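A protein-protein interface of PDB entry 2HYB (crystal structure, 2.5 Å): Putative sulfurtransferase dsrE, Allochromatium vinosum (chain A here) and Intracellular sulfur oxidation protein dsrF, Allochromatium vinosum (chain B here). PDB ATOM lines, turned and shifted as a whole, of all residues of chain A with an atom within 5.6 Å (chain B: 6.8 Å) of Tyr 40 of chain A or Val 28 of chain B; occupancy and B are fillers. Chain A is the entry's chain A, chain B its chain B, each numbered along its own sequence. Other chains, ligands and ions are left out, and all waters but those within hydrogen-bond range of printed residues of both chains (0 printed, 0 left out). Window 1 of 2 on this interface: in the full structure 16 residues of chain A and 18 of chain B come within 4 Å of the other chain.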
ATOM      1  N   GLN A   6      16.565 -14.862   5.614  1.00  0.00           N
ATOM      2  CA  GLN A   6      17.996 -14.686   5.338  1.00  0.00           C
ATOM      3  C   GLN A   6      18.185 -13.458   4.436  1.00  0.00           C
ATOM      4  O   GLN A   6      17.611 -13.382   3.348  1.00  0.00           O
ATOM      5  CB  GLN A   6      18.566 -15.931   4.642  1.00  0.00           C
ATOM      6  CG  GLN A   6      20.089 -15.959   4.511  1.00  0.00           C
ATOM      7  CD  GLN A   6      20.589 -17.156   3.735  1.00  0.00           C
ATOM      8  OE1 GLN A   6      19.999 -18.226   3.796  1.00  0.00           O
ATOM      9  NE2 GLN A   6      21.685 -16.982   3.010  1.00  0.00           N
ATOM     10  N   ILE A   7      18.990 -12.502   4.890  1.00  0.00           N
ATOM     11  CA  ILE A   7      19.246 -11.272   4.139  1.00  0.00           C
ATOM     12  C   ILE A   7      20.724 -11.182   3.789  1.00  0.00           C
ATOM     13  O   ILE A   7      21.568 -11.038   4.681  1.00  0.00           O
ATOM     14  CB  ILE A   7      18.855 -10.054   4.976  1.00  0.00           C
ATOM     15  CG1 ILE A   7      17.447 -10.259   5.525  1.00  0.00           C
ATOM     16  CG2 ILE A   7      18.920  -8.791   4.132  1.00  0.00           C
ATOM     17  CD1 ILE A   7      16.944  -9.100   6.365  1.00  0.00           C
ATOM     18  N   ASN A   8      21.038 -11.245   2.496  1.00  0.00           N
ATOM     19  CA  ASN A   8      22.439 -11.224   2.056  1.00  0.00           C
ATOM     20  C   ASN A   8      22.996  -9.897   1.589  1.00  0.00           C
ATOM     21  O   ASN A   8      24.158  -9.829   1.203  1.00  0.00           O
ATOM     22  CB  ASN A   8      22.668 -12.222   0.921  1.00  0.00           C
ATOM     23  CG  ASN A   8      22.023 -13.559   1.172  1.00  0.00           C
ATOM     24  OD1 ASN A   8      22.034 -14.070   2.295  1.00  0.00           O
ATOM     25  ND2 ASN A   8      21.472 -14.150   0.117  1.00  0.00           N
ATOM     26  N   GLU A   9      22.199  -8.842   1.606  1.00  0.00           N
ATOM     27  CA  GLU A   9      22.723  -7.570   1.132  1.00  0.00           C
ATOM     28  C   GLU A   9      22.649  -6.426   2.131  1.00  0.00           C
ATOM     29  O   GLU A   9      21.901  -6.472   3.112  1.00  0.00           O
ATOM     30  CB  GLU A   9      22.005  -7.155  -0.148  1.00  0.00           C
ATOM     31  CG  GLU A   9      21.936  -8.229  -1.231  1.00  0.00           C
ATOM     32  CD  GLU A   9      23.290  -8.612  -1.820  1.00  0.00           C
ATOM     33  OE1 GLU A   9      24.178  -7.736  -1.967  1.00  0.00           O
ATOM     34  OE2 GLU A   9      23.440  -9.803  -2.162  1.00  0.00           O
ATOM     35  N   PHE A  38      18.549 -13.703  10.029  1.00  0.00           N
ATOM     36  CA  PHE A  38      19.990 -13.876   9.919  1.00  0.00           C
ATOM     37  C   PHE A  38      20.609 -13.083   8.767  1.00  0.00           C
ATOM     38  O   PHE A  38      20.172 -13.204   7.618  1.00  0.00           O
ATOM     39  CB  PHE A  38      20.288 -15.371   9.766  1.00  0.00           C
ATOM     40  CG  PHE A  38      21.732 -15.718   9.878  1.00  0.00           C
ATOM     41  CD1 PHE A  38      22.595 -15.524   8.802  1.00  0.00           C
ATOM     42  CD2 PHE A  38      22.237 -16.236  11.062  1.00  0.00           C
ATOM     43  CE1 PHE A  38      23.941 -15.836   8.905  1.00  0.00           C
ATOM     44  CE2 PHE A  38      23.585 -16.550  11.177  1.00  0.00           C
ATOM     45  CZ  PHE A  38      24.435 -16.351  10.097  1.00  0.00           C
ATOM     46  N   PHE A  39      21.626 -12.278   9.086  1.00  0.00           N
ATOM     47  CA  PHE A  39      22.315 -11.459   8.096  1.00  0.00           C
ATOM     48  C   PHE A  39      23.638 -12.063   7.710  1.00  0.00           C
ATOM     49  O   PHE A  39      24.509 -12.245   8.550  1.00  0.00           O
ATOM     50  CB  PHE A  39      22.571 -10.061   8.630  1.00  0.00           C
ATOM     51  CG  PHE A  39      21.327  -9.294   8.936  1.00  0.00           C
ATOM     52  CD1 PHE A  39      20.695  -9.436  10.164  1.00  0.00           C
ATOM     53  CD2 PHE A  39      20.783  -8.415   7.999  1.00  0.00           C
ATOM     54  CE1 PHE A  39      19.534  -8.709  10.464  1.00  0.00           C
ATOM     55  CE2 PHE A  39      19.624  -7.687   8.291  1.00  0.00           C
ATOM     56  CZ  PHE A  39      19.003  -7.836   9.533  1.00  0.00           C
ATOM     57  N   TYR A  40      23.787 -12.357   6.427  1.00  0.00           N
ATOM     58  CA  TYR A  40      25.013 -12.939   5.905  1.00  0.00           C
ATOM     59  C   TYR A  40      25.522 -12.032   4.781  1.00  0.00           C
ATOM     60  O   TYR A  40      24.771 -11.182   4.310  1.00  0.00           O
ATOM     61  CB  TYR A  40      24.708 -14.348   5.398  1.00  0.00           C
ATOM     62  CG  TYR A  40      25.928 -15.187   5.163  1.00  0.00           C
ATOM     63  CD1 TYR A  40      27.007 -15.142   6.046  1.00  0.00           C
ATOM     64  CD2 TYR A  40      26.020 -16.024   4.053  1.00  0.00           C
ATOM     65  CE1 TYR A  40      28.142 -15.899   5.821  1.00  0.00           C
ATOM     66  CE2 TYR A  40      27.157 -16.787   3.829  1.00  0.00           C
ATOM     67  CZ  TYR A  40      28.213 -16.717   4.713  1.00  0.00           C
ATOM     68  OH  TYR A  40      29.355 -17.455   4.487  1.00  0.00           O
ATOM     69  N   HIS A  41      26.775 -12.203   4.348  1.00  0.00           N
ATOM     70  CA  HIS A  41      27.348 -11.354   3.293  1.00  0.00           C
ATOM     71  C   HIS A  41      27.163  -9.884   3.691  1.00  0.00           C
ATOM     72  O   HIS A  41      27.076  -9.558   4.877  1.00  0.00           O
ATOM     73  CB  HIS A  41      26.632 -11.564   1.954  1.00  0.00           C
ATOM     74  CG  HIS A  41      26.578 -12.988   1.493  1.00  0.00           C
ATOM     75  ND1 HIS A  41      27.690 -13.682   1.070  1.00  0.00           N
ATOM     76  CD2 HIS A  41      25.533 -13.839   1.365  1.00  0.00           C
ATOM     77  CE1 HIS A  41      27.332 -14.900   0.701  1.00  0.00           C
ATOM     78  NE2 HIS A  41      26.027 -15.019   0.870  1.00  0.00           N
ATOM     79  N   ASP A  42      27.093  -9.000   2.695  1.00  0.00           N
ATOM     80  CA  ASP A  42      26.881  -7.577   2.947  1.00  0.00           C
ATOM     81  C   ASP A  42      25.652  -7.369   3.846  1.00  0.00           C
ATOM     82  O   ASP A  42      25.428  -6.276   4.370  1.00  0.00           O
ATOM     83  CB  ASP A  42      26.703  -6.810   1.629  1.00  0.00           C
ATOM     84  CG  ASP A  42      28.022  -6.288   1.075  1.00  0.00           C
ATOM     85  OD1 ASP A  42      29.058  -6.467   1.751  1.00  0.00           O
ATOM     86  OD2 ASP A  42      28.028  -5.696  -0.028  1.00  0.00           O
ATOM     87  N   GLY A  43      24.859  -8.417   4.034  1.00  0.00           N
ATOM     88  CA  GLY A  43      23.702  -8.297   4.905  1.00  0.00           C
ATOM     89  C   GLY A  43      24.078  -7.838   6.317  1.00  0.00           C
ATOM     90  O   GLY A  43      23.341  -7.072   6.946  1.00  0.00           O
ATOM     91  N   VAL A  44      25.224  -8.289   6.825  1.00  0.00           N
ATOM     92  CA  VAL A  44      25.663  -7.903   8.156  1.00  0.00           C
ATOM     93  C   VAL A  44      25.728  -6.392   8.358  1.00  0.00           C
ATOM     94  O   VAL A  44      25.813  -5.922   9.487  1.00  0.00           O
ATOM     95  CB  VAL A  44      27.068  -8.479   8.475  1.00  0.00           C
ATOM     96  CG1 VAL A  44      27.023 -10.005   8.472  1.00  0.00           C
ATOM     97  CG2 VAL A  44      28.089  -7.951   7.469  1.00  0.00           C
ATOM     98  N   CYS A  78      26.271 -12.825  11.136  1.00  0.00           N
ATOM     99  CA  CYS A  78      27.367 -13.745  10.918  1.00  0.00           C
ATOM    100  C   CYS A  78      28.631 -13.060  11.378  1.00  0.00           C
ATOM    101  O   CYS A  78      28.919 -11.927  10.975  1.00  0.00           O
ATOM    102  CB  CYS A  78      27.503 -14.095   9.443  1.00  0.00           C
ATOM    103  SG  CYS A  78      28.848 -15.274   9.155  1.00  0.00           S
ATOM    104  N   ALA A  81      31.350 -12.953   8.532  1.00  0.00           N
ATOM    105  CA  ALA A  81      30.939 -11.959   7.554  1.00  0.00           C
ATOM    106  C   ALA A  81      31.245 -10.569   8.094  1.00  0.00           C
ATOM    107  O   ALA A  81      31.682  -9.688   7.356  1.00  0.00           O
ATOM    108  CB  ALA A  81      29.435 -12.100   7.266  1.00  0.00           C
ATOM    109  N   LEU A 112      27.688 -18.932  11.954  1.00  0.00           N
ATOM    110  CA  LEU A 112      26.968 -19.273  10.735  1.00  0.00           C
ATOM    111  C   LEU A 112      26.022 -20.426  11.065  1.00  0.00           C
ATOM    112  O   LEU A 112      25.000 -20.623  10.404  1.00  0.00           O
ATOM    113  CB  LEU A 112      27.963 -19.686   9.646  1.00  0.00           C
ATOM    114  CG  LEU A 112      27.445 -19.695   8.208  1.00  0.00           C
ATOM    115  CD1 LEU A 112      26.558 -18.473   7.976  1.00  0.00           C
ATOM    116  CD2 LEU A 112      28.622 -19.698   7.237  1.00  0.00           C
ATOM    117  N   LEU A 115      22.490 -19.894  11.354  1.00  0.00           N
ATOM    118  CA  LEU A 115      21.717 -19.793  10.133  1.00  0.00           C
ATOM    119  C   LEU A 115      21.127 -21.184   9.898  1.00  0.00           C
ATOM    120  O   LEU A 115      19.904 -21.345   9.819  1.00  0.00           O
ATOM    121  CB  LEU A 115      22.609 -19.388   8.950  1.00  0.00           C
ATOM    122  CG  LEU A 115      21.941 -19.495   7.570  1.00  0.00           C
ATOM    123  CD1 LEU A 115      20.673 -18.658   7.547  1.00  0.00           C
ATOM    124  CD2 LEU A 115      22.891 -19.051   6.484  1.00  0.00           C
ATOM    125  N   VAL A 116      21.997 -22.188   9.807  1.00  0.00           N
ATOM    126  CA  VAL A 116      21.565 -23.561   9.579  1.00  0.00           C
ATOM    127  C   VAL A 116      20.536 -23.998  10.637  1.00  0.00           C
ATOM    128  O   VAL A 116      19.517 -24.637  10.334  1.00  0.00           O
ATOM    129  CB  VAL A 116      22.784 -24.507   9.591  1.00  0.00           C
ATOM    130  CG1 VAL A 116      22.320 -25.954   9.478  1.00  0.00           C
ATOM    131  CG2 VAL A 116      23.723 -24.152   8.439  1.00  0.00           C
ATOM    132  N   TYR B  10      21.580 -26.498  -1.476  1.00  0.00           N
ATOM    133  CA  TYR B  10      22.415 -25.313  -1.552  1.00  0.00           C
ATOM    134  C   TYR B  10      22.524 -24.959  -3.020  1.00  0.00           C
ATOM    135  O   TYR B  10      23.324 -25.542  -3.759  1.00  0.00           O
ATOM    136  CB  TYR B  10      23.804 -25.587  -0.958  1.00  0.00           C
ATOM    137  CG  TYR B  10      23.824 -25.583   0.558  1.00  0.00           C
ATOM    138  CD1 TYR B  10      23.752 -24.390   1.271  1.00  0.00           C
ATOM    139  CD2 TYR B  10      23.870 -26.780   1.279  1.00  0.00           C
ATOM    140  CE1 TYR B  10      23.720 -24.390   2.655  1.00  0.00           C
ATOM    141  CE2 TYR B  10      23.836 -26.788   2.661  1.00  0.00           C
ATOM    142  CZ  TYR B  10      23.759 -25.594   3.345  1.00  0.00           C
ATOM    143  OH  TYR B  10      23.713 -25.609   4.720  1.00  0.00           O
ATOM    144  N   TYR B  21      29.757 -14.533  -3.197  1.00  0.00           N
ATOM    145  CA  TYR B  21      28.750 -15.571  -3.006  1.00  0.00           C
ATOM    146  C   TYR B  21      29.256 -17.000  -3.080  1.00  0.00           C
ATOM    147  O   TYR B  21      28.851 -17.840  -2.287  1.00  0.00           O
ATOM    148  CB  TYR B  21      27.597 -15.367  -3.984  1.00  0.00           C
ATOM    149  CG  TYR B  21      27.015 -13.984  -3.866  1.00  0.00           C
ATOM    150  CD1 TYR B  21      27.331 -13.004  -4.797  1.00  0.00           C
ATOM    151  CD2 TYR B  21      26.196 -13.634  -2.789  1.00  0.00           C
ATOM    152  CE1 TYR B  21      26.845 -11.709  -4.673  1.00  0.00           C
ATOM    153  CE2 TYR B  21      25.713 -12.338  -2.648  1.00  0.00           C
ATOM    154  CZ  TYR B  21      26.043 -11.379  -3.603  1.00  0.00           C
ATOM    155  OH  TYR B  21      25.567 -10.091  -3.499  1.00  0.00           O
ATOM    156  N   TRP B  23      32.341 -18.364  -2.414  1.00  0.00           N
ATOM    157  CA  TRP B  23      33.097 -18.620  -1.196  1.00  0.00           C
ATOM    158  C   TRP B  23      32.210 -18.699   0.047  1.00  0.00           C
ATOM    159  O   TRP B  23      32.113 -19.755   0.674  1.00  0.00           O
ATOM    160  CB  TRP B  23      34.142 -17.513  -1.033  1.00  0.00           C
ATOM    161  CG  TRP B  23      35.097 -17.656   0.122  1.00  0.00           C
ATOM    162  CD1 TRP B  23      35.771 -16.641   0.759  1.00  0.00           C
ATOM    163  CD2 TRP B  23      35.491 -18.867   0.782  1.00  0.00           C
ATOM    164  NE1 TRP B  23      36.548 -17.146   1.773  1.00  0.00           N
ATOM    165  CE2 TRP B  23      36.396 -18.507   1.808  1.00  0.00           C
ATOM    166  CE3 TRP B  23      35.170 -20.220   0.608  1.00  0.00           C
ATOM    167  CZ2 TRP B  23      36.982 -19.455   2.658  1.00  0.00           C
ATOM    168  CZ3 TRP B  23      35.755 -21.162   1.458  1.00  0.00           C
ATOM    169  CH2 TRP B  23      36.649 -20.771   2.467  1.00  0.00           C
ATOM    170  N   GLU B  24      31.551 -17.601   0.403  1.00  0.00           N
ATOM    171  CA  GLU B  24      30.724 -17.600   1.608  1.00  0.00           C
ATOM    172  C   GLU B  24      29.576 -18.624   1.622  1.00  0.00           C
ATOM    173  O   GLU B  24      29.084 -18.998   2.690  1.00  0.00           O
ATOM    174  CB  GLU B  24      30.234 -16.173   1.907  1.00  0.00           C
ATOM    175  CG  GLU B  24      31.411 -15.212   2.104  1.00  0.00           C
ATOM    176  CD  GLU B  24      31.043 -13.859   2.708  1.00  0.00           C
ATOM    177  OE1 GLU B  24      30.055 -13.240   2.270  1.00  0.00           O
ATOM    178  OE2 GLU B  24      31.767 -13.397   3.613  1.00  0.00           O
ATOM    179  N   ALA B  25      29.166 -19.094   0.447  1.00  0.00           N
ATOM    180  CA  ALA B  25      28.114 -20.107   0.361  1.00  0.00           C
ATOM    181  C   ALA B  25      28.760 -21.402   0.846  1.00  0.00           C
ATOM    182  O   ALA B  25      28.251 -22.065   1.749  1.00  0.00           O
ATOM    183  CB  ALA B  25      27.638 -20.264  -1.080  1.00  0.00           C
ATOM    184  N   LEU B  26      29.900 -21.728   0.241  1.00  0.00           N
ATOM    185  CA  LEU B  26      30.678 -22.911   0.587  1.00  0.00           C
ATOM    186  C   LEU B  26      30.853 -22.988   2.115  1.00  0.00           C
ATOM    187  O   LEU B  26      30.681 -24.052   2.717  1.00  0.00           O
ATOM    188  CB  LEU B  26      32.037 -22.840  -0.119  1.00  0.00           C
ATOM    189  CG  LEU B  26      32.988 -24.035  -0.029  1.00  0.00           C
ATOM    190  CD1 LEU B  26      32.246 -25.308  -0.359  1.00  0.00           C
ATOM    191  CD2 LEU B  26      34.158 -23.831  -0.977  1.00  0.00           C
ATOM    192  N   GLU B  27      31.175 -21.855   2.730  1.00  0.00           N
ATOM    193  CA  GLU B  27      31.344 -21.776   4.176  1.00  0.00           C
ATOM    194  C   GLU B  27      30.120 -22.359   4.901  1.00  0.00           C
ATOM    195  O   GLU B  27      30.247 -23.127   5.866  1.00  0.00           O
ATOM    196  CB  GLU B  27      31.505 -20.316   4.603  1.00  0.00           C
ATOM    197  CG  GLU B  27      32.697 -19.576   4.025  1.00  0.00           C
ATOM    198  CD  GLU B  27      33.985 -19.874   4.757  1.00  0.00           C
ATOM    199  OE1 GLU B  27      34.849 -18.975   4.831  1.00  0.00           O
ATOM    200  OE2 GLU B  27      34.136 -21.011   5.249  1.00  0.00           O
ATOM    201  N   VAL B  28      28.934 -21.976   4.433  1.00  0.00           N
ATOM    202  CA  VAL B  28      27.678 -22.436   5.024  1.00  0.00           C
ATOM    203  C   VAL B  28      27.504 -23.946   4.927  1.00  0.00           C
ATOM    204  O   VAL B  28      27.006 -24.583   5.853  1.00  0.00           O
ATOM    205  CB  VAL B  28      26.459 -21.781   4.341  1.00  0.00           C
ATOM    206  CG1 VAL B  28      25.178 -22.208   5.040  1.00  0.00           C
ATOM    207  CG2 VAL B  28      26.607 -20.277   4.372  1.00  0.00           C
ATOM    208  N   VAL B  29      27.895 -24.513   3.791  1.00  0.00           N
ATOM    209  CA  VAL B  29      27.779 -25.949   3.596  1.00  0.00           C
ATOM    210  C   VAL B  29      28.613 -26.637   4.676  1.00  0.00           C
ATOM    211  O   VAL B  29      28.117 -27.491   5.409  1.00  0.00           O
ATOM    212  CB  VAL B  29      28.277 -26.360   2.189  1.00  0.00           C
ATOM    213  CG1 VAL B  29      28.178 -27.868   2.017  1.00  0.00           C
ATOM    214  CG2 VAL B  29      27.450 -25.658   1.120  1.00  0.00           C
ATOM    215  N   LEU B  30      29.876 -26.234   4.785  1.00  0.00           N
ATOM    216  CA  LEU B  30      30.778 -26.808   5.772  1.00  0.00           C
ATOM    217  C   LEU B  30      30.191 -26.751   7.188  1.00  0.00           C
ATOM    218  O   LEU B  30      30.202 -27.748   7.913  1.00  0.00           O
ATOM    219  CB  LEU B  30      32.122 -26.082   5.730  1.00  0.00           C
ATOM    220  CG  LEU B  30      32.830 -26.055   4.373  1.00  0.00           C
ATOM    221  CD1 LEU B  30      34.232 -25.526   4.562  1.00  0.00           C
ATOM    222  CD2 LEU B  30      32.872 -27.445   3.773  1.00  0.00           C
ATOM    223  N   ILE B  31      29.677 -25.590   7.579  1.00  0.00           N
ATOM    224  CA  ILE B  31      29.086 -25.424   8.904  1.00  0.00           C
ATOM    225  C   ILE B  31      27.800 -26.232   9.111  1.00  0.00           C
ATOM    226  O   ILE B  31      27.514 -26.690  10.229  1.00  0.00           O
ATOM    227  CB  ILE B  31      28.801 -23.932   9.184  1.00  0.00           C
ATOM    228  CG1 ILE B  31      30.120 -23.227   9.467  1.00  0.00           C
ATOM    229  CG2 ILE B  31      27.869 -23.767  10.374  1.00  0.00           C
ATOM    230  CD1 ILE B  31      30.876 -23.840  10.633  1.00  0.00           C
ATOM    231  N   GLY B  32      27.028 -26.405   8.042  1.00  0.00           N
ATOM    232  CA  GLY B  32      25.784 -27.151   8.141  1.00  0.00           C
ATOM    233  C   GLY B  32      26.004 -28.649   8.144  1.00  0.00           C
ATOM    234  O   GLY B  32      25.100 -29.417   8.471  1.00  0.00           O
ATOM    235  N   ALA B  33      27.208 -29.066   7.772  1.00  0.00           N
ATOM    236  CA  ALA B  33      27.554 -30.480   7.731  1.00  0.00           C
ATOM    237  C   ALA B  33      27.414 -31.087   9.122  1.00  0.00           C
ATOM    238  O   ALA B  33      26.945 -32.218   9.280  1.00  0.00           O
ATOM    239  CB  ALA B  33      28.984 -30.644   7.236  1.00  0.00           C
ATOM    240  N   PHE B 134      18.887 -22.894   0.230  1.00  0.00           N
ATOM    241  CA  PHE B 134      19.727 -21.748   0.540  1.00  0.00           C
ATOM    242  C   PHE B 134      20.086 -21.142  -0.810  1.00  0.00           C
ATOM    243  O   PHE B 134      20.434 -21.876  -1.737  1.00  0.00           O
ATOM    244  CB  PHE B 134      20.990 -22.219   1.272  1.00  0.00           C
ATOM    245  CG  PHE B 134      20.720 -22.751   2.650  1.00  0.00           C
ATOM    246  CD1 PHE B 134      20.429 -21.880   3.691  1.00  0.00           C
ATOM    247  CD2 PHE B 134      20.716 -24.118   2.901  1.00  0.00           C
ATOM    248  CE1 PHE B 134      20.136 -22.360   4.963  1.00  0.00           C
ATOM    249  CE2 PHE B 134      20.423 -24.610   4.175  1.00  0.00           C
ATOM    250  CZ  PHE B 134      20.133 -23.733   5.206  1.00  0.00           C
ATOM    251  N   PHE B 136      22.206 -17.852  -2.987  1.00  0.00           N
ATOM    252  CA  PHE B 136      23.290 -16.888  -2.871  1.00  0.00           C
ATOM    253  C   PHE B 136      23.568 -16.201  -4.206  1.00  0.00           C
ATOM    254  O   PHE B 136      23.460 -14.980  -4.320  1.00  0.00           O
ATOM    255  CB  PHE B 136      24.569 -17.582  -2.382  1.00  0.00           C
ATOM    256  CG  PHE B 136      24.351 -18.525  -1.228  1.00  0.00           C
ATOM    257  CD1 PHE B 136      23.881 -19.815  -1.451  1.00  0.00           C
ATOM    258  CD2 PHE B 136      24.567 -18.116   0.082  1.00  0.00           C
ATOM    259  CE1 PHE B 136      23.625 -20.686  -0.387  1.00  0.00           C
ATOM    260  CE2 PHE B 136      24.316 -18.980   1.151  1.00  0.00           C
ATOM    261  CZ  PHE B 136      23.843 -20.265   0.918  1.00  0.00           C
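Of the 16 printed residues of chain A, 6 touch a printed residue of chain B.
Printed residues of chain A that touch a printed residue of chain B: Gln 6, Glu 9, Tyr 40, His 41, Leu 112 and Val 116.
Hydrophobic or aromatic side chains of chain A within 4 Å of the printed part of chain B: Tyr 40, His 41, Leu 112 and Val 116.
Hydrophobic or aromatic side chains of chain B that line the printed part of chain A: Tyr 10, Tyr 21, Val 28, Ile 31, Phe 134 and Phe 136.
Among the printed residues, 14 pairs touch across the chains.
The side-chain amide nitrogen (NE2) of Gln 6 of chain A lies within hydrogen-bond range of the side-chain amide oxygen (OD1) of Asn 8 of chain A (3.0 Å).
The backbone carbonyl oxygen (O) of Ile 7 of chain A sits at hydrogen-bond distance from the backbone NH (N) of Tyr 40 of chain A, 3.1 Å away.
Asn 8 of chain A touches none of the printed residues of chain B.
Printed residues of chain B within 4 Å of Glu 9 of chain A: Tyr 21.
Tyr 40 of chain A touches three residues of chain B.
Of the printed residues of chain B, Val 116 of chain A touches Tyr 10 and Gly 32.
Leu 26 of chain B touches none of the printed residues of chain A.
Val 28 of chain B touches two residues of chain A.
The nearest residue of chain B that does not touch Tyr 40 of chain A is Ala 25 of chain B (4.4 Å).
Gln 6 of chain A touches Phe 134 of chain B (OE1 to CD1, 3.7 Å).
Gln 6 of chain A touches Phe 136 of chain B.
Tyr 40 of chain A touches Glu 27 of chain B.
CE2 of Tyr 40 of chain A touches CG2 of Val 28 of chain B, at 3.6 Å.
His 41 of chain A touches Tyr 21 of chain B.
NE2 of His 41 of chain A touches CD2 of Phe 136 of chain B, at 3.5 Å.
Leu 112 of chain A touches Glu 27 of chain B (CD2 to C, 3.8 Å).
Leu 112 of chain A touches Val 28 of chain B.
Leu 112 of chain A touches Ile 31 of chain B.
Val 116 of chain A touches Gly 32 of chain B.
OE2 of Glu 9 of chain A is in hydrogen-bond range of OH of Tyr 21 of chain B, at 2.5 Å.
The side-chain carboxylate (OE1) of Glu 24 of chain B is in hydrogen-bond range of a ring nitrogen (ND1) of His 41 of chain A (2.7 Å).
OH of Tyr 40 of chain A sits close to O of Glu 24 of chain B (2.4 Å).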
